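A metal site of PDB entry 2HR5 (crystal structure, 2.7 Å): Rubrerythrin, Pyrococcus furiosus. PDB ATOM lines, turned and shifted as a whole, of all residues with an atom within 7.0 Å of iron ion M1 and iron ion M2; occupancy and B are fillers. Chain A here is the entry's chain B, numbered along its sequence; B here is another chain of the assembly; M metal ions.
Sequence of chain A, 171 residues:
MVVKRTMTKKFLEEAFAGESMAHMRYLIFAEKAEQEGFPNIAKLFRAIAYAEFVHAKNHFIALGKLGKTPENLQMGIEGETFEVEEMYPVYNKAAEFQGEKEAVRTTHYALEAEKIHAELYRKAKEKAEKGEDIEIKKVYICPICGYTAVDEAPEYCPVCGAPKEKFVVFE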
ATOM      1  N   GLY A  76       8.987  -5.501   8.020  1.00  0.00           N
ATOM      2  CA  GLY A  76      10.072  -5.836   7.080  1.00  0.00           C
ATOM      3  C   GLY A  76      11.450  -5.325   7.466  1.00  0.00           C
ATOM      4  O   GLY A  76      12.455  -6.104   7.463  1.00  0.00           O
ATOM      5  N   GLY A  79      12.651  -7.242  10.662  1.00  0.00           N
ATOM      6  CA  GLY A  79      13.111  -8.499  10.156  1.00  0.00           C
ATOM      7  C   GLY A  79      14.513  -8.450   9.538  1.00  0.00           C
ATOM      8  O   GLY A  79      15.447  -9.190   9.966  1.00  0.00           O
ATOM      9  N   GLU A  80      14.679  -7.608   8.531  1.00  0.00           N
ATOM     10  CA  GLU A  80      15.931  -7.589   7.759  1.00  0.00           C
ATOM     11  C   GLU A  80      17.113  -7.101   8.609  1.00  0.00           C
ATOM     12  O   GLU A  80      18.277  -7.639   8.544  1.00  0.00           O
ATOM     13  CB  GLU A  80      15.779  -6.663   6.551  1.00  0.00           C
ATOM     14  CG  GLU A  80      14.649  -7.076   5.536  1.00  0.00           C
ATOM     15  CD  GLU A  80      14.967  -8.352   4.743  1.00  0.00           C
ATOM     16  OE1 GLU A  80      16.146  -8.871   4.797  1.00  0.00           O
ATOM     17  OE2 GLU A  80      14.014  -8.875   4.174  1.00  0.00           O
ATOM     18  N   GLU A  83      18.324  -9.674  10.895  1.00  0.00           N
ATOM     19  CA  GLU A  83      19.144 -10.598  10.156  1.00  0.00           C
ATOM     20  C   GLU A  83      20.482 -10.076   9.795  1.00  0.00           C
ATOM     21  O   GLU A  83      21.436 -10.832   9.880  1.00  0.00           O
ATOM     22  CB  GLU A  83      18.421 -11.007   8.923  1.00  0.00           C
ATOM     23  CG  GLU A  83      17.304 -11.946   9.239  1.00  0.00           C
ATOM     24  CD  GLU A  83      16.419 -12.156   8.075  1.00  0.00           C
ATOM     25  OE1 GLU A  83      16.710 -11.567   7.011  1.00  0.00           O
ATOM     26  OE2 GLU A  83      15.424 -12.903   8.216  1.00  0.00           O
ATOM     27  N   TYR A  88      22.495 -13.493  10.832  1.00  0.00           N
ATOM     28  CA  TYR A  88      23.313 -14.101   9.803  1.00  0.00           C
ATOM     29  C   TYR A  88      24.814 -13.969  10.085  1.00  0.00           C
ATOM     30  O   TYR A  88      25.549 -14.937   9.829  1.00  0.00           O
ATOM     31  CB  TYR A  88      22.900 -13.704   8.371  1.00  0.00           C
ATOM     32  CG  TYR A  88      21.748 -14.543   7.765  1.00  0.00           C
ATOM     33  CD1 TYR A  88      21.811 -15.974   7.712  1.00  0.00           C
ATOM     34  CD2 TYR A  88      20.617 -13.921   7.219  1.00  0.00           C
ATOM     35  CE1 TYR A  88      20.757 -16.740   7.153  1.00  0.00           C
ATOM     36  CE2 TYR A  88      19.560 -14.639   6.643  1.00  0.00           C
ATOM     37  CZ  TYR A  88      19.634 -16.063   6.610  1.00  0.00           C
ATOM     38  OH  TYR A  88      18.572 -16.794   6.073  1.00  0.00           O
ATOM     39  N   TYR A 109      25.507 -15.625   1.289  1.00  0.00           N
ATOM     40  CA  TYR A 109      24.551 -15.210   0.270  1.00  0.00           C
ATOM     41  C   TYR A 109      23.327 -14.513   0.913  1.00  0.00           C
ATOM     42  O   TYR A 109      22.902 -13.432   0.471  1.00  0.00           O
ATOM     43  CB  TYR A 109      24.110 -16.400  -0.521  1.00  0.00           C
ATOM     44  CG  TYR A 109      25.054 -17.017  -1.561  1.00  0.00           C
ATOM     45  CD1 TYR A 109      26.220 -16.404  -1.965  1.00  0.00           C
ATOM     46  CD2 TYR A 109      24.684 -18.195  -2.202  1.00  0.00           C
ATOM     47  CE1 TYR A 109      27.051 -17.007  -2.931  1.00  0.00           C
ATOM     48  CE2 TYR A 109      25.444 -18.786  -3.123  1.00  0.00           C
ATOM     49  CZ  TYR A 109      26.639 -18.204  -3.508  1.00  0.00           C
ATOM     50  OH  TYR A 109      27.371 -18.860  -4.485  1.00  0.00           O
ATOM     51  N   ALA A 110      22.749 -15.082   1.964  1.00  0.00           N
ATOM     52  CA  ALA A 110      21.550 -14.422   2.540  1.00  0.00           C
ATOM     53  C   ALA A 110      21.866 -13.004   3.162  1.00  0.00           C
ATOM     54  O   ALA A 110      21.140 -12.033   2.872  1.00  0.00           O
ATOM     55  CB  ALA A 110      20.849 -15.319   3.549  1.00  0.00           C
ATOM     56  N   LEU A 111      22.893 -12.946   4.030  1.00  0.00           N
ATOM     57  CA  LEU A 111      23.373 -11.712   4.680  1.00  0.00           C
ATOM     58  C   LEU A 111      23.521 -10.564   3.678  1.00  0.00           C
ATOM     59  O   LEU A 111      22.832  -9.533   3.809  1.00  0.00           O
ATOM     60  CB  LEU A 111      24.704 -11.979   5.412  1.00  0.00           C
ATOM     61  CG  LEU A 111      25.348 -10.834   6.264  1.00  0.00           C
ATOM     62  CD1 LEU A 111      24.235 -10.093   7.018  1.00  0.00           C
ATOM     63  CD2 LEU A 111      26.493 -11.348   7.227  1.00  0.00           C
ATOM     64  N   ALA A 113      22.280 -10.198   0.694  1.00  0.00           N
ATOM     65  CA  ALA A 113      20.924  -9.791   0.248  1.00  0.00           C
ATOM     66  C   ALA A 113      20.063  -9.057   1.286  1.00  0.00           C
ATOM     67  O   ALA A 113      19.235  -8.157   0.908  1.00  0.00           O
ATOM     68  CB  ALA A 113      20.113 -10.942  -0.371  1.00  0.00           C
ATOM     69  N   GLU A 114      20.224  -9.410   2.559  1.00  0.00           N
ATOM     70  CA  GLU A 114      19.430  -8.705   3.569  1.00  0.00           C
ATOM     71  C   GLU A 114      19.812  -7.241   3.722  1.00  0.00           C
ATOM     72  O   GLU A 114      18.925  -6.415   3.940  1.00  0.00           O
ATOM     73  CB  GLU A 114      19.405  -9.383   4.947  1.00  0.00           C
ATOM     74  CG  GLU A 114      19.343 -10.891   5.006  1.00  0.00           C
ATOM     75  CD  GLU A 114      18.292 -11.540   4.081  1.00  0.00           C
ATOM     76  OE1 GLU A 114      18.174 -12.751   4.180  1.00  0.00           O
ATOM     77  OE2 GLU A 114      17.692 -10.887   3.263  1.00  0.00           O
ATOM     78  N   LYS A 115      21.106  -6.925   3.572  1.00  0.00           N
ATOM     79  CA  LYS A 115      21.530  -5.520   3.670  1.00  0.00           C
ATOM     80  C   LYS A 115      20.716  -4.729   2.693  1.00  0.00           C
ATOM     81  O   LYS A 115      20.084  -3.720   3.071  1.00  0.00           O
ATOM     82  CB  LYS A 115      23.010  -5.354   3.388  1.00  0.00           C
ATOM     83  CG  LYS A 115      23.775  -5.956   4.510  1.00  0.00           C
ATOM     84  CD  LYS A 115      25.121  -6.218   4.117  1.00  0.00           C
ATOM     85  CE  LYS A 115      25.898  -6.740   5.270  1.00  0.00           C
ATOM     86  NZ  LYS A 115      27.216  -7.159   4.638  1.00  0.00           N
ATOM     87  N   HIS A 117      17.921  -5.520   1.268  1.00  0.00           N
ATOM     88  CA  HIS A 117      16.470  -5.525   1.539  1.00  0.00           C
ATOM     89  C   HIS A 117      16.079  -4.481   2.604  1.00  0.00           C
ATOM     90  O   HIS A 117      15.121  -3.697   2.423  1.00  0.00           O
ATOM     91  CB  HIS A 117      15.964  -6.908   1.921  1.00  0.00           C
ATOM     92  CG  HIS A 117      16.138  -7.957   0.846  1.00  0.00           C
ATOM     93  ND1 HIS A 117      16.005  -9.303   1.087  1.00  0.00           N
ATOM     94  CD2 HIS A 117      16.442  -7.844  -0.470  1.00  0.00           C
ATOM     95  CE1 HIS A 117      16.191  -9.980  -0.033  1.00  0.00           C
ATOM     96  NE2 HIS A 117      16.469  -9.116  -0.988  1.00  0.00           N
ATOM     97  N   ALA A 118      16.827  -4.472   3.721  1.00  0.00           N
ATOM     98  CA  ALA A 118      16.696  -3.438   4.775  1.00  0.00           C
ATOM     99  C   ALA A 118      16.618  -2.026   4.165  1.00  0.00           C
ATOM    100  O   ALA A 118      15.596  -1.354   4.392  1.00  0.00           O
ATOM    101  CB  ALA A 118      17.808  -3.533   5.819  1.00  0.00           C
ATOM    102  N   TYR A 121      13.391  -1.241   2.018  1.00  0.00           N
ATOM    103  CA  TYR A 121      12.109  -1.145   2.680  1.00  0.00           C
ATOM    104  C   TYR A 121      12.053   0.222   3.418  1.00  0.00           C
ATOM    105  O   TYR A 121      10.999   0.899   3.504  1.00  0.00           O
ATOM    106  CB  TYR A 121      11.960  -2.341   3.627  1.00  0.00           C
ATOM    107  CG  TYR A 121      11.547  -3.660   3.027  1.00  0.00           C
ATOM    108  CD1 TYR A 121      12.108  -4.862   3.476  1.00  0.00           C
ATOM    109  CD2 TYR A 121      10.598  -3.705   2.004  1.00  0.00           C
ATOM    110  CE1 TYR A 121      11.658  -6.148   2.912  1.00  0.00           C
ATOM    111  CE2 TYR A 121      10.156  -4.907   1.419  1.00  0.00           C
ATOM    112  CZ  TYR A 121      10.671  -6.131   1.870  1.00  0.00           C
ATOM    113  OH  TYR A 121      10.142  -7.284   1.270  1.00  0.00           O
ATOM    114  N   GLY B  18      13.138 -19.137   9.210  1.00  0.00           N
ATOM    115  CA  GLY B  18      13.109 -17.683   9.118  1.00  0.00           C
ATOM    116  C   GLY B  18      12.936 -17.216   7.680  1.00  0.00           C
ATOM    117  O   GLY B  18      12.161 -16.280   7.430  1.00  0.00           O
ATOM    118  N   GLU B  19      13.593 -17.826   6.706  1.00  0.00           N
ATOM    119  CA  GLU B  19      13.386 -17.367   5.334  1.00  0.00           C
ATOM    120  C   GLU B  19      11.984 -17.700   4.845  1.00  0.00           C
ATOM    121  O   GLU B  19      11.361 -16.934   4.093  1.00  0.00           O
ATOM    122  CB  GLU B  19      14.435 -17.896   4.335  1.00  0.00           C
ATOM    123  CG  GLU B  19      15.849 -17.462   4.651  1.00  0.00           C
ATOM    124  CD  GLU B  19      16.090 -16.026   4.240  1.00  0.00           C
ATOM    125  OE1 GLU B  19      17.262 -15.635   4.235  1.00  0.00           O
ATOM    126  OE2 GLU B  19      15.073 -15.328   3.949  1.00  0.00           O
ATOM    127  N   ALA B  22       9.751 -15.055   6.353  1.00  0.00           N
ATOM    128  CA  ALA B  22       9.957 -13.805   5.654  1.00  0.00           C
ATOM    129  C   ALA B  22       9.236 -13.808   4.230  1.00  0.00           C
ATOM    130  O   ALA B  22       8.463 -12.863   3.919  1.00  0.00           O
ATOM    131  CB  ALA B  22      11.415 -13.490   5.595  1.00  0.00           C
ATOM    132  N   TYR B  26       6.087 -11.382   3.214  1.00  0.00           N
ATOM    133  CA  TYR B  26       6.178 -10.544   2.029  1.00  0.00           C
ATOM    134  C   TYR B  26       5.108 -10.758   1.008  1.00  0.00           C
ATOM    135  O   TYR B  26       4.608  -9.789   0.421  1.00  0.00           O
ATOM    136  CB  TYR B  26       7.514 -10.691   1.365  1.00  0.00           C
ATOM    137  CG  TYR B  26       8.599 -10.238   2.325  1.00  0.00           C
ATOM    138  CD1 TYR B  26       9.933 -10.494   2.072  1.00  0.00           C
ATOM    139  CD2 TYR B  26       8.257  -9.614   3.527  1.00  0.00           C
ATOM    140  CE1 TYR B  26      10.923 -10.094   2.957  1.00  0.00           C
ATOM    141  CE2 TYR B  26       9.217  -9.212   4.449  1.00  0.00           C
ATOM    142  CZ  TYR B  26      10.550  -9.469   4.165  1.00  0.00           C
ATOM    143  OH  TYR B  26      11.509  -9.100   5.089  1.00  0.00           O
ATOM    144  N   ILE B  48      11.265  -9.304  -3.464  1.00  0.00           N
ATOM    145  CA  ILE B  48      11.984  -9.743  -2.247  1.00  0.00           C
ATOM    146  C   ILE B  48      11.508 -11.121  -1.721  1.00  0.00           C
ATOM    147  O   ILE B  48      12.333 -11.965  -1.316  1.00  0.00           O
ATOM    148  CB  ILE B  48      12.103  -8.635  -1.200  1.00  0.00           C
ATOM    149  CG1 ILE B  48      12.907  -7.467  -1.834  1.00  0.00           C
ATOM    150  CG2 ILE B  48      12.771  -9.174   0.091  1.00  0.00           C
ATOM    151  CD1 ILE B  48      12.803  -6.073  -1.081  1.00  0.00           C
ATOM    152  N   ALA B  51      13.608 -13.507  -3.536  1.00  0.00           N
ATOM    153  CA  ALA B  51      14.931 -13.574  -2.895  1.00  0.00           C
ATOM    154  C   ALA B  51      14.882 -14.496  -1.718  1.00  0.00           C
ATOM    155  O   ALA B  51      15.860 -15.225  -1.493  1.00  0.00           O
ATOM    156  CB  ALA B  51      15.417 -12.223  -2.443  1.00  0.00           C
ATOM    157  N   GLU B  52      13.769 -14.504  -0.975  1.00  0.00           N
ATOM    158  CA  GLU B  52      13.814 -15.288   0.279  1.00  0.00           C
ATOM    159  C   GLU B  52      13.671 -16.775   0.042  1.00  0.00           C
ATOM    160  O   GLU B  52      14.224 -17.586   0.780  1.00  0.00           O
ATOM    161  CB  GLU B  52      12.762 -14.818   1.294  1.00  0.00           C
ATOM    162  CG  GLU B  52      12.568 -13.334   1.319  1.00  0.00           C
ATOM    163  CD  GLU B  52      13.794 -12.566   1.831  1.00  0.00           C
ATOM    164  OE1 GLU B  52      13.575 -11.542   2.507  1.00  0.00           O
ATOM    165  OE2 GLU B  52      14.919 -12.934   1.568  1.00  0.00           O
ATOM    166  N   PHE B  53      12.844 -17.082  -0.979  1.00  0.00           N
ATOM    167  CA  PHE B  53      12.696 -18.407  -1.527  1.00  0.00           C
ATOM    168  C   PHE B  53      14.074 -18.892  -2.008  1.00  0.00           C
ATOM    169  O   PHE B  53      14.425 -20.084  -1.817  1.00  0.00           O
ATOM    170  CB  PHE B  53      11.744 -18.375  -2.728  1.00  0.00           C
ATOM    171  CG  PHE B  53      11.979 -19.500  -3.687  1.00  0.00           C
ATOM    172  CD1 PHE B  53      11.432 -20.737  -3.457  1.00  0.00           C
ATOM    173  CD2 PHE B  53      12.818 -19.348  -4.789  1.00  0.00           C
ATOM    174  CE1 PHE B  53      11.602 -21.747  -4.321  1.00  0.00           C
ATOM    175  CE2 PHE B  53      13.021 -20.368  -5.662  1.00  0.00           C
ATOM    176  CZ  PHE B  53      12.408 -21.590  -5.428  1.00  0.00           C
ATOM    177  N   VAL B  54      14.854 -17.989  -2.639  1.00  0.00           N
ATOM    178  CA  VAL B  54      16.177 -18.366  -3.060  1.00  0.00           C
ATOM    179  C   VAL B  54      17.055 -18.666  -1.850  1.00  0.00           C
ATOM    180  O   VAL B  54      17.742 -19.684  -1.819  1.00  0.00           O
ATOM    181  CB  VAL B  54      16.832 -17.373  -4.068  1.00  0.00           C
ATOM    182  CG1 VAL B  54      18.291 -17.753  -4.342  1.00  0.00           C
ATOM    183  CG2 VAL B  54      16.121 -17.462  -5.381  1.00  0.00           C
ATOM    184  N   HIS B  55      17.021 -17.846  -0.829  1.00  0.00           N
ATOM    185  CA  HIS B  55      17.833 -18.218   0.351  1.00  0.00           C
ATOM    186  C   HIS B  55      17.345 -19.465   1.031  1.00  0.00           C
ATOM    187  O   HIS B  55      18.134 -20.314   1.492  1.00  0.00           O
ATOM    188  CB  HIS B  55      17.827 -17.119   1.362  1.00  0.00           C
ATOM    189  CG  HIS B  55      18.262 -15.827   0.808  1.00  0.00           C
ATOM    190  ND1 HIS B  55      17.787 -14.640   1.286  1.00  0.00           N
ATOM    191  CD2 HIS B  55      19.110 -15.527  -0.212  1.00  0.00           C
ATOM    192  CE1 HIS B  55      18.331 -13.640   0.612  1.00  0.00           C
ATOM    193  NE2 HIS B  55      19.141 -14.146  -0.303  1.00  0.00           N
ATOM    194  N   ALA B  56      16.027 -19.606   1.086  1.00  0.00           N
ATOM    195  CA  ALA B  56      15.484 -20.745   1.825  1.00  0.00           C
ATOM    196  C   ALA B  56      15.890 -21.965   1.023  1.00  0.00           C
ATOM    197  O   ALA B  56      16.410 -22.932   1.618  1.00  0.00           O
ATOM    198  CB  ALA B  56      13.952 -20.661   2.028  1.00  0.00           C
ATOM    199  N   HIS B  59      19.454 -22.852   1.810  1.00  0.00           N
ATOM    200  CA  HIS B  59      19.627 -23.515   3.119  1.00  0.00           C
ATOM    201  C   HIS B  59      19.180 -24.975   3.072  1.00  0.00           C
ATOM    202  O   HIS B  59      19.906 -25.843   3.580  1.00  0.00           O
ATOM    203  CB  HIS B  59      18.913 -22.799   4.257  1.00  0.00           C
ATOM    204  CG  HIS B  59      19.338 -21.382   4.421  1.00  0.00           C
ATOM    205  ND1 HIS B  59      20.633 -20.963   4.217  1.00  0.00           N
ATOM    206  CD2 HIS B  59      18.645 -20.290   4.832  1.00  0.00           C
ATOM    207  CE1 HIS B  59      20.712 -19.669   4.441  1.00  0.00           C
ATOM    208  NE2 HIS B  59      19.513 -19.224   4.810  1.00  0.00           N
HETATM  209 FE    FE M   1      15.497 -10.393   3.126  1.00  0.00          FE
HETATM  210 FE    FE M   2      16.509 -13.811   3.034  1.00  0.00          FE
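Within 4 Å of iron ion M1: Glu 80, Glu 114, His 117 and Glu 52 of chain B. The nearest printed residue that does not touch iron ion M1 is Glu 83 (4.2 Å).
Iron ion M2 is bound by OE2 of Glu 19 of chain B (2.3 Å), OE1 of Glu 114 (2.3 Å), OE1 of Glu 19 of chain B (2.3 Å), ND1 of His 55 of chain B (2.3 Å) and OE2 of Glu 52 of chain B (2.3 Å). Iron ion M2 has five donor atoms within binding distance.
The side-chain carboxylate of Glu 19 of chain B lies close to the side-chain hydroxyl of Tyr 88, at 2.5 Å. ND1 of His 55 of chain B sits close to O of Ala 51 of chain B (3.4 Å). The side-chain carboxylate (OE2) of Glu 80 lies close to the side-chain hydroxyl (OH) of Tyr 26 of chain B (2.7 Å). A ring nitrogen (NE2) of His 117 sits close to the backbone carbonyl oxygen of Ala 113, 3.5 Å away.
Iron ion M1 is bound by OE2 of Glu 114 (2.3 Å), OE1 of Glu 52 of chain B (2.3 Å), OE1 of Glu 80 (2.4 Å), OE2 of Glu 80 (2.4 Å) and ND1 of His 117 (2.4 Å).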
